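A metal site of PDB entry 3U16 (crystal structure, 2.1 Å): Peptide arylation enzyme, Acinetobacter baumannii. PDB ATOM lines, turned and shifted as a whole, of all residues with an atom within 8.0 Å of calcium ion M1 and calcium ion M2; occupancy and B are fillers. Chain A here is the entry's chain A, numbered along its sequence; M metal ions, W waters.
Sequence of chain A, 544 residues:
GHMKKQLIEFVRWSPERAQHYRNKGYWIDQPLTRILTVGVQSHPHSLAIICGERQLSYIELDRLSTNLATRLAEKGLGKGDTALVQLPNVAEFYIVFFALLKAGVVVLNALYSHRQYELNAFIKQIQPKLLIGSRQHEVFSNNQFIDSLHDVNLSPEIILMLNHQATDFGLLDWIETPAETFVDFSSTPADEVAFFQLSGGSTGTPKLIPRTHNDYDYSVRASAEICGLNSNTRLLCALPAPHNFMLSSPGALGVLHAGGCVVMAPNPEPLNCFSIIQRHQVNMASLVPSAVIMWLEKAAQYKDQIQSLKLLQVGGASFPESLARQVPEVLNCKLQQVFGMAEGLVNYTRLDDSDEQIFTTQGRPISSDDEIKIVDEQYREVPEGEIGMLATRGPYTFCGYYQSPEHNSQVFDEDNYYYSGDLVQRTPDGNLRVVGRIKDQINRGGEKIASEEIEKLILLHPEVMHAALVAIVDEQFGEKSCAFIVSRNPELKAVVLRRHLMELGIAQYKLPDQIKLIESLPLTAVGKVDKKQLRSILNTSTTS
Within 4 Å of calcium ion M2: Glu 329 and Asn 332.
The nearest printed residue that does not touch calcium ion M2 is Pro 328 (4.02 Å).
Three residues have an atom within 4 Å of calcium ion M1: Gln 307, Leu 309 and Asn 332.
The nearest printed residue that does not touch calcium ion M1 is Ser 308 (4.3 Å).
N of Asn 332 is in hydrogen-bond range of O of Val 327 (3.2 Å).
OD1 of Asn 332 lies close to O of Val 330.
Calcium ion M2 is bound by the side-chain amide oxygen of Asn 332 (2.5 Å), the backbone carbonyl oxygen of Glu 329 (2.5 Å), water W2 (2.6 Å), water W1 (2.7 Å) and water W3 (2.7 Å).
Water W4 bridges O of Leu 331 and O of Ile 306.
Calcium ion M1 is bound by O of Gln 307 (2.4 Å), O of Leu 309 (2.5 Å), water W4 (2.5 Å), water W6 (2.5 Å) and O of Asn 332 (2.5 Å).
Calcium ion M1 has five donor atoms within binding distance.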
ATOM      1  N   VAL A 282      -2.355 -25.331  13.898  1.00  0.00           N
ATOM      2  CA  VAL A 282      -1.744 -24.139  13.319  1.00  0.00           C
ATOM      3  C   VAL A 282      -2.495 -23.712  12.060  1.00  0.00           C
ATOM      4  O   VAL A 282      -2.817 -24.544  11.205  1.00  0.00           O
ATOM      5  CB  VAL A 282      -0.274 -24.402  12.955  1.00  0.00           C
ATOM      6  CG1 VAL A 282       0.273 -23.271  12.075  1.00  0.00           C
ATOM      7  CG2 VAL A 282       0.556 -24.590  14.221  1.00  0.00           C
ATOM      8  N   ASN A 283      -2.793 -22.416  11.924  1.00  0.00           N
ATOM      9  CA  ASN A 283      -3.501 -21.980  10.727  1.00  0.00           C
ATOM     10  C   ASN A 283      -2.736 -21.023   9.825  1.00  0.00           C
ATOM     11  O   ASN A 283      -3.227 -20.648   8.769  1.00  0.00           O
ATOM     12  CB  ASN A 283      -4.893 -21.437  11.065  1.00  0.00           C
ATOM     13  CG  ASN A 283      -4.877 -20.387  12.164  1.00  0.00           C
ATOM     14  OD1 ASN A 283      -3.906 -19.634  12.311  1.00  0.00           O
ATOM     15  ND2 ASN A 283      -5.954 -20.322  12.919  1.00  0.00           N
ATOM     16  N   LYS A 303      -1.237 -35.039   4.191  1.00  0.00           N
ATOM     17  CA  LYS A 303      -2.344 -34.132   3.930  1.00  0.00           C
ATOM     18  C   LYS A 303      -3.182 -33.874   5.190  1.00  0.00           C
ATOM     19  O   LYS A 303      -3.487 -32.726   5.520  1.00  0.00           O
ATOM     20  CB  LYS A 303      -3.210 -34.709   2.813  1.00  0.00           C
ATOM     21  CG  LYS A 303      -4.296 -33.788   2.325  1.00  0.00           C
ATOM     22  CD  LYS A 303      -4.929 -34.328   1.052  1.00  0.00           C
ATOM     23  CE  LYS A 303      -5.385 -35.765   1.208  1.00  0.00           C
ATOM     24  NZ  LYS A 303      -4.390 -36.746   0.657  1.00  0.00           N
ATOM     25  N   ILE A 306      -1.750 -31.331   7.909  1.00  0.00           N
ATOM     26  CA  ILE A 306      -1.616 -29.907   7.640  1.00  0.00           C
ATOM     27  C   ILE A 306      -2.890 -29.240   7.135  1.00  0.00           C
ATOM     28  O   ILE A 306      -2.869 -28.084   6.730  1.00  0.00           O
ATOM     29  CB  ILE A 306      -0.472 -29.611   6.654  1.00  0.00           C
ATOM     30  CG1 ILE A 306      -0.849 -30.079   5.255  1.00  0.00           C
ATOM     31  CG2 ILE A 306       0.816 -30.279   7.118  1.00  0.00           C
ATOM     32  CD1 ILE A 306       0.192 -29.735   4.232  1.00  0.00           C
ATOM     33  N   GLN A 307      -4.017 -29.953   7.182  1.00  0.00           N
ATOM     34  CA  GLN A 307      -5.259 -29.382   6.687  1.00  0.00           C
ATOM     35  C   GLN A 307      -5.582 -28.019   7.321  1.00  0.00           C
ATOM     36  O   GLN A 307      -6.129 -27.132   6.666  1.00  0.00           O
ATOM     37  CB  GLN A 307      -6.418 -30.358   6.892  1.00  0.00           C
ATOM     38  CG  GLN A 307      -6.477 -30.907   8.306  1.00  0.00           C
ATOM     39  CD  GLN A 307      -7.654 -31.841   8.534  1.00  0.00           C
ATOM     40  OE1 GLN A 307      -8.815 -31.426   8.444  1.00  0.00           O
ATOM     41  NE2 GLN A 307      -7.350 -33.105   8.868  1.00  0.00           N
ATOM     42  N   SER A 308      -5.236 -27.843   8.602  1.00  0.00           N
ATOM     43  CA  SER A 308      -5.629 -26.605   9.287  1.00  0.00           C
ATOM     44  C   SER A 308      -4.939 -25.343   8.740  1.00  0.00           C
ATOM     45  O   SER A 308      -5.413 -24.238   8.984  1.00  0.00           O
ATOM     46  CB  SER A 308      -5.451 -26.723  10.804  1.00  0.00           C
ATOM     47  OG  SER A 308      -4.086 -26.832  11.181  1.00  0.00           O
ATOM     48  N   LEU A 309      -3.852 -25.486   7.985  1.00  0.00           N
ATOM     49  CA  LEU A 309      -3.173 -24.302   7.450  1.00  0.00           C
ATOM     50  C   LEU A 309      -4.140 -23.476   6.603  1.00  0.00           C
ATOM     51  O   LEU A 309      -4.750 -24.010   5.704  1.00  0.00           O
ATOM     52  CB  LEU A 309      -1.979 -24.700   6.566  1.00  0.00           C
ATOM     53  CG  LEU A 309      -0.677 -25.151   7.216  1.00  0.00           C
ATOM     54  CD1 LEU A 309       0.367 -25.339   6.145  1.00  0.00           C
ATOM     55  CD2 LEU A 309      -0.198 -24.120   8.267  1.00  0.00           C
ATOM     56  N   LYS A 310      -4.275 -22.177   6.863  1.00  0.00           N
ATOM     57  CA  LYS A 310      -5.149 -21.360   6.020  1.00  0.00           C
ATOM     58  C   LYS A 310      -4.343 -20.379   5.178  1.00  0.00           C
ATOM     59  O   LYS A 310      -4.804 -19.922   4.127  1.00  0.00           O
ATOM     60  CB  LYS A 310      -6.139 -20.562   6.863  1.00  0.00           C
ATOM     61  CG  LYS A 310      -7.181 -21.373   7.604  1.00  0.00           C
ATOM     62  CD  LYS A 310      -8.083 -20.419   8.381  1.00  0.00           C
ATOM     63  CE  LYS A 310      -9.017 -21.135   9.334  1.00  0.00           C
ATOM     64  NZ  LYS A 310      -9.850 -20.127  10.065  1.00  0.00           N
ATOM     65  N   LEU A 311      -3.160 -20.024   5.653  1.00  0.00           N
ATOM     66  CA  LEU A 311      -2.358 -19.025   4.945  1.00  0.00           C
ATOM     67  C   LEU A 311      -0.882 -19.346   5.099  1.00  0.00           C
ATOM     68  O   LEU A 311      -0.408 -19.626   6.197  1.00  0.00           O
ATOM     69  CB  LEU A 311      -2.656 -17.618   5.472  1.00  0.00           C
ATOM     70  CG  LEU A 311      -1.855 -16.462   4.859  1.00  0.00           C
ATOM     71  CD1 LEU A 311      -2.038 -16.393   3.352  1.00  0.00           C
ATOM     72  CD2 LEU A 311      -2.229 -15.117   5.518  1.00  0.00           C
ATOM     73  N   GLN A 326       1.740 -24.409  -6.794  1.00  0.00           N
ATOM     74  CA  GLN A 326       1.665 -25.657  -6.033  1.00  0.00           C
ATOM     75  C   GLN A 326       1.249 -25.452  -4.573  1.00  0.00           C
ATOM     76  O   GLN A 326       0.862 -26.410  -3.901  1.00  0.00           O
ATOM     77  CB  GLN A 326       2.987 -26.421  -6.086  1.00  0.00           C
ATOM     78  CG  GLN A 326       3.363 -26.911  -7.487  1.00  0.00           C
ATOM     79  CD  GLN A 326       4.714 -27.612  -7.513  1.00  0.00           C
ATOM     80  OE1 GLN A 326       4.933 -28.597  -6.780  1.00  0.00           O
ATOM     81  NE2 GLN A 326       5.627 -27.126  -8.359  1.00  0.00           N
ATOM     82  N   VAL A 327       1.322 -24.223  -4.072  1.00  0.00           N
ATOM     83  CA  VAL A 327       0.999 -23.997  -2.661  1.00  0.00           C
ATOM     84  C   VAL A 327      -0.485 -24.282  -2.347  1.00  0.00           C
ATOM     85  O   VAL A 327      -0.776 -25.152  -1.535  1.00  0.00           O
ATOM     86  CB  VAL A 327       1.426 -22.583  -2.191  1.00  0.00           C
ATOM     87  CG1 VAL A 327       0.811 -22.248  -0.841  1.00  0.00           C
ATOM     88  CG2 VAL A 327       2.961 -22.505  -2.144  1.00  0.00           C
ATOM     89  N   PRO A 328      -1.411 -23.579  -3.024  1.00  0.00           N
ATOM     90  CA  PRO A 328      -2.828 -23.862  -2.774  1.00  0.00           C
ATOM     91  C   PRO A 328      -3.167 -25.269  -3.213  1.00  0.00           C
ATOM     92  O   PRO A 328      -3.974 -25.938  -2.578  1.00  0.00           O
ATOM     93  CB  PRO A 328      -3.566 -22.870  -3.692  1.00  0.00           C
ATOM     94  CG  PRO A 328      -2.521 -21.974  -4.267  1.00  0.00           C
ATOM     95  CD  PRO A 328      -1.208 -22.653  -4.142  1.00  0.00           C
ATOM     96  N   GLU A 329      -2.543 -25.711  -4.313  1.00  0.00           N
ATOM     97  CA  GLU A 329      -2.832 -27.016  -4.889  1.00  0.00           C
ATOM     98  C   GLU A 329      -2.404 -28.170  -4.000  1.00  0.00           C
ATOM     99  O   GLU A 329      -3.133 -29.148  -3.841  1.00  0.00           O
ATOM    100  CB  GLU A 329      -2.129 -27.157  -6.257  1.00  0.00           C
ATOM    101  CG  GLU A 329      -2.372 -28.493  -6.940  1.00  0.00           C
ATOM    102  CD  GLU A 329      -3.768 -28.587  -7.557  1.00  0.00           C
ATOM    103  OE1 GLU A 329      -4.230 -27.575  -8.118  1.00  0.00           O
ATOM    104  OE2 GLU A 329      -4.382 -29.679  -7.484  1.00  0.00           O
ATOM    105  N   VAL A 330      -1.218 -28.077  -3.421  1.00  0.00           N
ATOM    106  CA  VAL A 330      -0.681 -29.199  -2.651  1.00  0.00           C
ATOM    107  C   VAL A 330      -0.760 -28.978  -1.142  1.00  0.00           C
ATOM    108  O   VAL A 330      -1.110 -29.895  -0.383  1.00  0.00           O
ATOM    109  CB  VAL A 330       0.767 -29.504  -3.050  1.00  0.00           C
ATOM    110  CG1 VAL A 330       1.342 -30.573  -2.130  1.00  0.00           C
ATOM    111  CG2 VAL A 330       0.830 -29.952  -4.517  1.00  0.00           C
ATOM    112  N   LEU A 331      -0.437 -27.764  -0.684  1.00  0.00           N
ATOM    113  CA  LEU A 331      -0.456 -27.477   0.748  1.00  0.00           C
ATOM    114  C   LEU A 331      -1.853 -27.068   1.210  1.00  0.00           C
ATOM    115  O   LEU A 331      -2.115 -26.909   2.404  1.00  0.00           O
ATOM    116  CB  LEU A 331       0.571 -26.379   1.099  1.00  0.00           C
ATOM    117  CG  LEU A 331       2.050 -26.738   0.864  1.00  0.00           C
ATOM    118  CD1 LEU A 331       2.986 -25.590   1.257  1.00  0.00           C
ATOM    119  CD2 LEU A 331       2.413 -28.009   1.639  1.00  0.00           C
ATOM    120  N   ASN A 332      -2.755 -26.879   0.250  1.00  0.00           N
ATOM    121  CA  ASN A 332      -4.167 -26.626   0.564  1.00  0.00           C
ATOM    122  C   ASN A 332      -4.396 -25.383   1.423  1.00  0.00           C
ATOM    123  O   ASN A 332      -5.215 -25.382   2.318  1.00  0.00           O
ATOM    124  CB  ASN A 332      -4.790 -27.870   1.230  1.00  0.00           C
ATOM    125  CG  ASN A 332      -4.690 -29.104   0.328  1.00  0.00           C
ATOM    126  OD1 ASN A 332      -4.369 -28.974  -0.830  1.00  0.00           O
ATOM    127  ND2 ASN A 332      -4.915 -30.281   0.876  1.00  0.00           N
ATOM    128  N   CYS A 333      -3.665 -24.316   1.130  1.00  0.00           N
ATOM    129  CA  CYS A 333      -3.900 -23.071   1.846  1.00  0.00           C
ATOM    130  C   CYS A 333      -3.661 -21.920   0.881  1.00  0.00           C
ATOM    131  O   CYS A 333      -3.038 -22.087  -0.166  1.00  0.00           O
ATOM    132  CB  CYS A 333      -2.960 -22.958   3.039  1.00  0.00           C
ATOM    133  SG  CYS A 333      -1.217 -23.114   2.541  1.00  0.00           S
ATOM    134  N   LYS A 334      -4.146 -20.742   1.253  1.00  0.00           N
ATOM    135  CA  LYS A 334      -3.878 -19.558   0.460  1.00  0.00           C
ATOM    136  C   LYS A 334      -2.388 -19.194   0.490  1.00  0.00           C
ATOM    137  O   LYS A 334      -1.694 -19.449   1.489  1.00  0.00           O
ATOM    138  CB  LYS A 334      -4.739 -18.401   0.964  1.00  0.00           C
ATOM    139  CG  LYS A 334      -4.176 -17.023   0.624  1.00  0.00           C
ATOM    140  CD  LYS A 334      -5.019 -16.303  -0.408  1.00  0.00           C
ATOM    141  CE  LYS A 334      -6.290 -15.756   0.236  1.00  0.00           C
ATOM    142  NZ  LYS A 334      -7.143 -15.057  -0.761  1.00  0.00           N
HETATM  143 CA    CA M   1      -6.063 -25.795   4.650  1.00  0.00          CA
HETATM  144 CA    CA M   2      -5.415 -29.675  -2.934  1.00  0.00          CA
HETATM  145  O   HOH W   1      -6.901 -29.783  -5.156  1.00  0.00           O
HETATM  146  O   HOH W   2      -4.930 -31.910  -4.240  1.00  0.00           O
HETATM  147  O   HOH W   3      -6.468 -27.233  -3.302  1.00  0.00           O
HETATM  148  O   HOH W   4      -3.861 -26.964   4.435  1.00  0.00           O
HETATM  149  O   HOH W   5      -4.200 -32.185  -1.454  1.00  0.00           O
HETATM  150  O   HOH W   6      -7.626 -27.472   3.625  1.00  0.00           O
